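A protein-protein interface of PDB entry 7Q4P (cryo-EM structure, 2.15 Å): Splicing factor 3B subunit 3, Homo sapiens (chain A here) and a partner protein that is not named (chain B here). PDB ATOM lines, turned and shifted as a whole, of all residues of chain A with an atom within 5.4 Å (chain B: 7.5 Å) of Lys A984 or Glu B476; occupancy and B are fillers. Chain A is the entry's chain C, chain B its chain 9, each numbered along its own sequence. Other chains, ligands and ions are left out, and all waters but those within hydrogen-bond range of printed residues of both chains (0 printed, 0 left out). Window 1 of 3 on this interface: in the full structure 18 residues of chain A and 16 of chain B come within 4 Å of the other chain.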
ATOM      1  N   LYS A 965     -37.963 -32.239 -31.887  1.00  0.00           N
ATOM      2  CA  LYS A 965     -37.935 -32.886 -30.582  1.00  0.00           C
ATOM      3  C   LYS A 965     -37.007 -32.165 -29.594  1.00  0.00           C
ATOM      4  O   LYS A 965     -36.695 -32.712 -28.514  1.00  0.00           O
ATOM      5  CB  LYS A 965     -37.354 -34.280 -30.787  1.00  0.00           C
ATOM      6  CG  LYS A 965     -35.873 -34.363 -31.096  1.00  0.00           C
ATOM      7  CD  LYS A 965     -35.581 -35.657 -31.819  1.00  0.00           C
ATOM      8  CE  LYS A 965     -34.966 -36.682 -30.897  1.00  0.00           C
ATOM      9  NZ  LYS A 965     -33.640 -36.193 -30.464  1.00  0.00           N
ATOM     10  N   LEU A 966     -36.545 -30.967 -29.963  1.00  0.00           N
ATOM     11  CA  LEU A 966     -35.645 -30.220 -29.081  1.00  0.00           C
ATOM     12  C   LEU A 966     -36.425 -29.137 -28.376  1.00  0.00           C
ATOM     13  O   LEU A 966     -37.149 -28.405 -29.060  1.00  0.00           O
ATOM     14  CB  LEU A 966     -34.578 -29.513 -29.907  1.00  0.00           C
ATOM     15  CG  LEU A 966     -33.820 -30.451 -30.815  1.00  0.00           C
ATOM     16  CD1 LEU A 966     -33.122 -29.667 -31.907  1.00  0.00           C
ATOM     17  CD2 LEU A 966     -32.789 -31.244 -30.026  1.00  0.00           C
ATOM     18  N   ARG A 979     -30.690 -18.671 -28.824  1.00  0.00           N
ATOM     19  CA  ARG A 979     -30.828 -19.926 -28.110  1.00  0.00           C
ATOM     20  C   ARG A 979     -30.021 -19.900 -26.813  1.00  0.00           C
ATOM     21  O   ARG A 979     -28.818 -19.701 -26.843  1.00  0.00           O
ATOM     22  CB  ARG A 979     -30.364 -21.090 -28.983  1.00  0.00           C
ATOM     23  CG  ARG A 979     -30.446 -22.411 -28.233  1.00  0.00           C
ATOM     24  CD  ARG A 979     -30.004 -23.689 -28.885  1.00  0.00           C
ATOM     25  NE  ARG A 979     -28.861 -23.500 -29.750  1.00  0.00           N
ATOM     26  CZ  ARG A 979     -28.402 -24.439 -30.552  1.00  0.00           C
ATOM     27  NH1 ARG A 979     -28.991 -25.626 -30.583  1.00  0.00           N
ATOM     28  NH2 ARG A 979     -27.356 -24.199 -31.322  1.00  0.00           N
ATOM     29  N   GLU A 982     -31.073 -25.826 -24.013  1.00  0.00           N
ATOM     30  CA  GLU A 982     -31.678 -26.878 -24.811  1.00  0.00           C
ATOM     31  C   GLU A 982     -31.763 -28.161 -23.986  1.00  0.00           C
ATOM     32  O   GLU A 982     -30.859 -28.471 -23.216  1.00  0.00           O
ATOM     33  CB  GLU A 982     -30.884 -27.065 -26.099  1.00  0.00           C
ATOM     34  CG  GLU A 982     -31.640 -27.840 -27.147  1.00  0.00           C
ATOM     35  CD  GLU A 982     -30.921 -27.879 -28.476  1.00  0.00           C
ATOM     36  OE1 GLU A 982     -31.056 -26.909 -29.262  1.00  0.00           O
ATOM     37  OE2 GLU A 982     -30.245 -28.879 -28.747  1.00  0.00           O
ATOM     38  N   ASN A 983     -32.844 -28.926 -24.172  1.00  0.00           N
ATOM     39  CA  ASN A 983     -32.890 -30.327 -23.806  1.00  0.00           C
ATOM     40  C   ASN A 983     -33.039 -31.126 -25.097  1.00  0.00           C
ATOM     41  O   ASN A 983     -33.874 -30.786 -25.938  1.00  0.00           O
ATOM     42  CB  ASN A 983     -34.021 -30.594 -22.811  1.00  0.00           C
ATOM     43  CG  ASN A 983     -34.023 -32.019 -22.306  1.00  0.00           C
ATOM     44  OD1 ASN A 983     -34.350 -32.961 -23.024  1.00  0.00           O
ATOM     45  ND2 ASN A 983     -33.572 -32.235 -21.091  1.00  0.00           N
ATOM     46  N   LYS A 984     -32.254 -32.213 -25.235  1.00  0.00           N
ATOM     47  CA  LYS A 984     -32.311 -33.053 -26.425  1.00  0.00           C
ATOM     48  C   LYS A 984     -32.883 -34.449 -26.164  1.00  0.00           C
ATOM     49  O   LYS A 984     -32.928 -35.282 -27.065  1.00  0.00           O
ATOM     50  CB  LYS A 984     -30.911 -33.197 -27.004  1.00  0.00           C
ATOM     51  CG  LYS A 984     -30.266 -31.872 -27.355  1.00  0.00           C
ATOM     52  CD  LYS A 984     -28.892 -32.047 -27.988  1.00  0.00           C
ATOM     53  CE  LYS A 984     -28.037 -30.790 -28.018  1.00  0.00           C
ATOM     54  NZ  LYS A 984     -28.242 -29.965 -26.805  1.00  0.00           N
ATOM     55  N   HIS A 985     -33.399 -34.707 -24.955  1.00  0.00           N
ATOM     56  CA  HIS A 985     -33.814 -36.044 -24.542  1.00  0.00           C
ATOM     57  C   HIS A 985     -35.303 -36.344 -24.783  1.00  0.00           C
ATOM     58  O   HIS A 985     -35.772 -37.428 -24.426  1.00  0.00           O
ATOM     59  CB  HIS A 985     -33.394 -36.277 -23.083  1.00  0.00           C
ATOM     60  CG  HIS A 985     -31.946 -35.994 -22.804  1.00  0.00           C
ATOM     61  ND1 HIS A 985     -31.570 -34.865 -22.140  1.00  0.00           N
ATOM     62  CD2 HIS A 985     -30.791 -36.653 -23.114  1.00  0.00           C
ATOM     63  CE1 HIS A 985     -30.254 -34.853 -21.991  1.00  0.00           C
ATOM     64  NE2 HIS A 985     -29.750 -35.937 -22.587  1.00  0.00           N
ATOM     65  N   ILE A 986     -36.069 -35.417 -25.389  1.00  0.00           N
ATOM     66  CA  ILE A 986     -37.464 -35.687 -25.738  1.00  0.00           C
ATOM     67  C   ILE A 986     -37.520 -36.708 -26.879  1.00  0.00           C
ATOM     68  O   ILE A 986     -36.779 -36.614 -27.858  1.00  0.00           O
ATOM     69  CB  ILE A 986     -38.287 -34.406 -26.032  1.00  0.00           C
ATOM     70  CG1 ILE A 986     -38.094 -33.289 -24.994  1.00  0.00           C
ATOM     71  CG2 ILE A 986     -39.765 -34.728 -26.237  1.00  0.00           C
ATOM     72  CD1 ILE A 986     -38.604 -33.593 -23.593  1.00  0.00           C
ATOM     73  N   ALA B 467     -22.084 -36.861 -26.050  1.00  0.00           N
ATOM     74  CA  ALA B 467     -21.708 -35.469 -26.249  1.00  0.00           C
ATOM     75  C   ALA B 467     -22.709 -34.762 -27.162  1.00  0.00           C
ATOM     76  O   ALA B 467     -22.894 -33.551 -27.068  1.00  0.00           O
ATOM     77  CB  ALA B 467     -20.302 -35.374 -26.790  1.00  0.00           C
ATOM     78  N   SER B 468     -23.360 -35.537 -28.034  1.00  0.00           N
ATOM     79  CA  SER B 468     -24.391 -35.060 -28.946  1.00  0.00           C
ATOM     80  C   SER B 468     -25.762 -35.071 -28.269  1.00  0.00           C
ATOM     81  O   SER B 468     -26.743 -34.584 -28.833  1.00  0.00           O
ATOM     82  CB  SER B 468     -24.386 -35.897 -30.204  1.00  0.00           C
ATOM     83  OG  SER B 468     -25.297 -35.396 -31.173  1.00  0.00           O
ATOM     84  N   GLU B 469     -25.831 -35.690 -27.085  1.00  0.00           N
ATOM     85  CA  GLU B 469     -27.045 -35.767 -26.286  1.00  0.00           C
ATOM     86  C   GLU B 469     -27.152 -34.476 -25.476  1.00  0.00           C
ATOM     87  O   GLU B 469     -28.255 -33.985 -25.228  1.00  0.00           O
ATOM     88  CB  GLU B 469     -27.051 -37.052 -25.460  1.00  0.00           C
ATOM     89  CG  GLU B 469     -27.764 -38.215 -26.136  1.00  0.00           C
ATOM     90  CD  GLU B 469     -27.772 -39.517 -25.351  1.00  0.00           C
ATOM     91  OE1 GLU B 469     -28.213 -39.507 -24.182  1.00  0.00           O
ATOM     92  OE2 GLU B 469     -27.326 -40.536 -25.911  1.00  0.00           O
ATOM     93  N   ARG B 470     -26.000 -34.003 -24.988  1.00  0.00           N
ATOM     94  CA  ARG B 470     -25.956 -33.099 -23.856  1.00  0.00           C
ATOM     95  C   ARG B 470     -25.836 -31.659 -24.340  1.00  0.00           C
ATOM     96  O   ARG B 470     -25.457 -31.407 -25.487  1.00  0.00           O
ATOM     97  CB  ARG B 470     -24.892 -33.512 -22.835  1.00  0.00           C
ATOM     98  CG  ARG B 470     -23.477 -33.058 -23.169  1.00  0.00           C
ATOM     99  CD  ARG B 470     -22.519 -33.333 -22.027  1.00  0.00           C
ATOM    100  NE  ARG B 470     -21.366 -32.440 -22.038  1.00  0.00           N
ATOM    101  CZ  ARG B 470     -21.280 -31.284 -21.383  1.00  0.00           C
ATOM    102  NH1 ARG B 470     -22.288 -30.850 -20.642  1.00  0.00           N
ATOM    103  NH2 ARG B 470     -20.178 -30.561 -21.471  1.00  0.00           N
ATOM    104  N   TRP B 471     -26.308 -30.773 -23.463  1.00  0.00           N
ATOM    105  CA  TRP B 471     -26.342 -29.328 -23.617  1.00  0.00           C
ATOM    106  C   TRP B 471     -24.946 -28.759 -23.368  1.00  0.00           C
ATOM    107  O   TRP B 471     -24.359 -29.004 -22.320  1.00  0.00           O
ATOM    108  CB  TRP B 471     -27.396 -28.771 -22.646  1.00  0.00           C
ATOM    109  CG  TRP B 471     -27.321 -27.303 -22.351  1.00  0.00           C
ATOM    110  CD1 TRP B 471     -27.213 -26.741 -21.117  1.00  0.00           C
ATOM    111  CD2 TRP B 471     -27.365 -26.190 -23.289  1.00  0.00           C
ATOM    112  NE1 TRP B 471     -27.218 -25.374 -21.219  1.00  0.00           N
ATOM    113  CE2 TRP B 471     -27.269 -24.991 -22.542  1.00  0.00           C
ATOM    114  CE3 TRP B 471     -27.465 -26.069 -24.687  1.00  0.00           C
ATOM    115  CZ2 TRP B 471     -27.277 -23.722 -23.157  1.00  0.00           C
ATOM    116  CZ3 TRP B 471     -27.486 -24.822 -25.298  1.00  0.00           C
ATOM    117  CH2 TRP B 471     -27.365 -23.652 -24.540  1.00  0.00           C
ATOM    118  N   GLN B 472     -24.408 -28.029 -24.355  1.00  0.00           N
ATOM    119  CA  GLN B 472     -23.026 -27.599 -24.346  1.00  0.00           C
ATOM    120  C   GLN B 472     -23.003 -26.071 -24.323  1.00  0.00           C
ATOM    121  O   GLN B 472     -23.063 -25.446 -25.360  1.00  0.00           O
ATOM    122  CB  GLN B 472     -22.314 -28.125 -25.596  1.00  0.00           C
ATOM    123  CG  GLN B 472     -22.254 -29.643 -25.786  1.00  0.00           C
ATOM    124  CD  GLN B 472     -21.059 -30.303 -25.141  1.00  0.00           C
ATOM    125  OE1 GLN B 472     -20.485 -29.808 -24.173  1.00  0.00           O
ATOM    126  NE2 GLN B 472     -20.677 -31.451 -25.676  1.00  0.00           N
ATOM    127  N   PRO B 473     -23.194 -25.415 -23.164  1.00  0.00           N
ATOM    128  CA  PRO B 473     -23.487 -23.980 -23.161  1.00  0.00           C
ATOM    129  C   PRO B 473     -22.309 -23.080 -23.514  1.00  0.00           C
ATOM    130  O   PRO B 473     -22.456 -21.856 -23.543  1.00  0.00           O
ATOM    131  CB  PRO B 473     -23.901 -23.729 -21.713  1.00  0.00           C
ATOM    132  CG  PRO B 473     -23.160 -24.782 -20.914  1.00  0.00           C
ATOM    133  CD  PRO B 473     -23.142 -25.994 -21.819  1.00  0.00           C
ATOM    134  N   ASP B 474     -21.158 -23.727 -23.749  1.00  0.00           N
ATOM    135  CA  ASP B 474     -19.876 -23.087 -23.992  1.00  0.00           C
ATOM    136  C   ASP B 474     -19.716 -22.796 -25.482  1.00  0.00           C
ATOM    137  O   ASP B 474     -18.986 -21.879 -25.846  1.00  0.00           O
ATOM    138  CB  ASP B 474     -18.712 -23.901 -23.412  1.00  0.00           C
ATOM    139  CG  ASP B 474     -18.740 -24.013 -21.895  1.00  0.00           C
ATOM    140  OD1 ASP B 474     -19.212 -23.058 -21.240  1.00  0.00           O
ATOM    141  OD2 ASP B 474     -18.288 -25.052 -21.380  1.00  0.00           O
ATOM    142  N   THR B 475     -20.481 -23.523 -26.306  1.00  0.00           N
ATOM    143  CA  THR B 475     -20.403 -23.374 -27.750  1.00  0.00           C
ATOM    144  C   THR B 475     -21.786 -23.201 -28.389  1.00  0.00           C
ATOM    145  O   THR B 475     -21.906 -22.736 -29.520  1.00  0.00           O
ATOM    146  CB  THR B 475     -19.591 -24.524 -28.358  1.00  0.00           C
ATOM    147  OG1 THR B 475     -19.410 -24.251 -29.746  1.00  0.00           O
ATOM    148  CG2 THR B 475     -20.249 -25.873 -28.177  1.00  0.00           C
ATOM    149  N   GLU B 476     -22.832 -23.549 -27.638  1.00  0.00           N
ATOM    150  CA  GLU B 476     -24.161 -23.710 -28.189  1.00  0.00           C
ATOM    151  C   GLU B 476     -25.038 -22.541 -27.754  1.00  0.00           C
ATOM    152  O   GLU B 476     -26.034 -22.292 -28.427  1.00  0.00           O
ATOM    153  CB  GLU B 476     -24.698 -25.086 -27.798  1.00  0.00           C
ATOM    154  CG  GLU B 476     -25.554 -25.756 -28.847  1.00  0.00           C
ATOM    155  CD  GLU B 476     -25.861 -27.225 -28.601  1.00  0.00           C
ATOM    156  OE1 GLU B 476     -26.050 -27.957 -29.592  1.00  0.00           O
ATOM    157  OE2 GLU B 476     -25.917 -27.642 -27.420  1.00  0.00           O
ATOM    158  N   GLU B 477     -24.719 -21.890 -26.604  1.00  0.00           N
ATOM    159  CA  GLU B 477     -25.394 -20.651 -26.216  1.00  0.00           C
ATOM    160  C   GLU B 477     -24.982 -19.524 -27.153  1.00  0.00           C
ATOM    161  O   GLU B 477     -23.812 -19.392 -27.522  1.00  0.00           O
ATOM    162  CB  GLU B 477     -24.956 -20.085 -24.864  1.00  0.00           C
ATOM    163  CG  GLU B 477     -25.821 -20.612 -23.760  1.00  0.00           C
ATOM    164  CD  GLU B 477     -25.564 -19.898 -22.455  1.00  0.00           C
ATOM    165  OE1 GLU B 477     -26.011 -18.746 -22.329  1.00  0.00           O
ATOM    166  OE2 GLU B 477     -24.903 -20.497 -21.579  1.00  0.00           O
ATOM    167  N   GLU B 478     -26.000 -18.754 -27.526  1.00  0.00           N
ATOM    168  CA  GLU B 478     -25.903 -17.723 -28.536  1.00  0.00           C
ATOM    169  C   GLU B 478     -25.996 -16.403 -27.798  1.00  0.00           C
ATOM    170  O   GLU B 478     -26.809 -16.254 -26.892  1.00  0.00           O
ATOM    171  CB  GLU B 478     -27.057 -17.835 -29.530  1.00  0.00           C
ATOM    172  CG  GLU B 478     -26.984 -19.058 -30.428  1.00  0.00           C
ATOM    173  CD  GLU B 478     -28.018 -19.153 -31.534  1.00  0.00           C
ATOM    174  OE1 GLU B 478     -29.199 -18.837 -31.274  1.00  0.00           O
ATOM    175  OE2 GLU B 478     -27.634 -19.543 -32.657  1.00  0.00           O
ATOM    176  N   TYR B 479     -25.081 -15.501 -28.139  1.00  0.00           N
ATOM    177  CA  TYR B 479     -24.981 -14.197 -27.516  1.00  0.00           C
ATOM    178  C   TYR B 479     -24.928 -13.121 -28.595  1.00  0.00           C
ATOM    179  O   TYR B 479     -24.599 -13.406 -29.741  1.00  0.00           O
ATOM    180  CB  TYR B 479     -23.717 -14.172 -26.660  1.00  0.00           C
ATOM    181  CG  TYR B 479     -23.858 -14.841 -25.318  1.00  0.00           C
ATOM    182  CD1 TYR B 479     -23.483 -16.167 -25.104  1.00  0.00           C
ATOM    183  CD2 TYR B 479     -24.367 -14.121 -24.248  1.00  0.00           C
ATOM    184  CE1 TYR B 479     -23.607 -16.750 -23.846  1.00  0.00           C
ATOM    185  CE2 TYR B 479     -24.484 -14.688 -22.990  1.00  0.00           C
ATOM    186  CZ  TYR B 479     -24.101 -16.002 -22.784  1.00  0.00           C
ATOM    187  OH  TYR B 479     -24.235 -16.505 -21.521  1.00  0.00           O
ATOM    188  N   VAL B 487     -22.642 -14.505 -31.453  1.00  0.00           N
ATOM    189  CA  VAL B 487     -21.357 -14.950 -30.934  1.00  0.00           C
ATOM    190  C   VAL B 487     -21.571 -15.974 -29.824  1.00  0.00           C
ATOM    191  O   VAL B 487     -22.633 -16.002 -29.216  1.00  0.00           O
ATOM    192  CB  VAL B 487     -20.491 -13.775 -30.434  1.00  0.00           C
ATOM    193  CG1 VAL B 487     -19.792 -13.071 -31.579  1.00  0.00           C
ATOM    194  CG2 VAL B 487     -21.210 -12.799 -29.507  1.00  0.00           C
ATOM    195  N   ASN B 488     -20.544 -16.790 -29.547  1.00  0.00           N
ATOM    196  CA  ASN B 488     -20.561 -17.751 -28.455  1.00  0.00           C
ATOM    197  C   ASN B 488     -20.020 -17.103 -27.180  1.00  0.00           C
ATOM    198  O   ASN B 488     -19.633 -15.934 -27.181  1.00  0.00           O
ATOM    199  CB  ASN B 488     -19.841 -19.053 -28.826  1.00  0.00           C
ATOM    200  CG  ASN B 488     -18.345 -18.895 -29.013  1.00  0.00           C
ATOM    201  OD1 ASN B 488     -17.886 -18.139 -29.869  1.00  0.00           O
ATOM    202  ND2 ASN B 488     -17.569 -19.623 -28.232  1.00  0.00           N
ATOM    203  N   LYS B 489     -20.019 -17.888 -26.096  1.00  0.00           N
ATOM    204  CA  LYS B 489     -19.773 -17.406 -24.745  1.00  0.00           C
ATOM    205  C   LYS B 489     -18.305 -17.012 -24.578  1.00  0.00           C
ATOM    206  O   LYS B 489     -17.992 -16.149 -23.758  1.00  0.00           O
ATOM    207  CB  LYS B 489     -20.145 -18.477 -23.720  1.00  0.00           C
ATOM    208  CG  LYS B 489     -20.502 -17.932 -22.343  1.00  0.00           C
ATOM    209  CD  LYS B 489     -21.235 -18.920 -21.455  1.00  0.00           C
ATOM    210  CE  LYS B 489     -20.321 -19.859 -20.693  1.00  0.00           C
ATOM    211  NZ  LYS B 489     -21.089 -20.821 -19.869  1.00  0.00           N
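The backbone carbonyl oxygen (O) of Arg B470 is in hydrogen-bond range of the side-chain amino group (NZ) of Lys A984 (3.4 Å).
The side-chain amino group of Lys A984 is in salt-bridge range of the side-chain carboxylate of Glu B476, at 3.3 Å.
The side-chain carboxylate of Glu B478 sits at hydrogen-bond distance from the backbone NH of Arg A979 (2.9 Å).
NH1 of Arg A979 lies within salt-bridge range of OE1 of Glu B476, at 3.9 Å.
The side-chain amino group (NZ) of Lys A984 is in salt-bridge range of the side-chain carboxylate (OE2) of Glu A982 (3.0 Å).
NH1 of Arg A979 lies within salt-bridge range of OE1 of Glu A982, at 2.8 Å.
The side-chain carboxylate of Glu B477 is in hydrogen-bond range of the side-chain hydroxyl of Tyr B479 (3.0 Å).
The side-chain amide oxygen (OD1) of Asn A983 sits at hydrogen-bond distance from the backbone NH (N) of His A985 (2.8 Å).
The backbone NH (N) of Gln B472 sits at hydrogen-bond distance from the side-chain carboxylate (OE2) of Glu B476, 3.4 Å away.
OE1 of Gln B472 sits at hydrogen-bond distance from NH2 of Arg B470 (2.8 Å).
Arg A979 touches Glu B477.
CB of Trp B471 touches O of Glu A982 (3.5 Å).
O of Ser B468 touches CD of Lys A984, at 3.4 Å.
Lys A984 touches Glu B469.
NZ of Lys A984 touches CA of Trp B471, 3.8 Å away.
His A985 touches Glu B469 (NE2 to O, 3.6 Å).
Lys A984 touches five residues of chain B.
Glu B476 touches just these residues of chain A: Arg A979 (3.3 Å) and Lys A984 (3.3 Å).
Of the printed residues of chain B, Arg A979 touches Glu B476, Glu B477 and Glu B478.
Printed residues of chain A within 4 Å of Ser B468: Lys A984 (3.4 Å).
Of the printed residues of chain A, Trp B471 touches Glu A982 and Lys A984.
Of the printed residues of chain B, His A985 touches Glu B469.
Of the printed residues of chain B, Glu A982 touches Trp B471 (3.5 Å).
Lys A965 touches none of the printed residues of chain B.
Pro B473 touches none of the printed residues of chain A.
The nearest residue of chain B that does not touch Lys A984 is Gln B472 (4.9 Å).
The nearest residue of chain A that does not touch Glu B476 is Glu A982 (4.4 Å).
Hydrophobic or aromatic side chains of chain A that line the printed part of chain B: His A985.
Of the 16 printed residues of chain B, 7 touch a printed residue of chain A.
Printed residues of chain B that touch a printed residue of chain A: Ser B468, Glu B469, Arg B470, Trp B471, Glu B476, Glu B477 and Glu B478.
Hydrophobic or aromatic side chains of chain B within 4 Å of the printed part of chain A: Trp B471.
Among the printed residues, 10 pairs touch across the chains.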
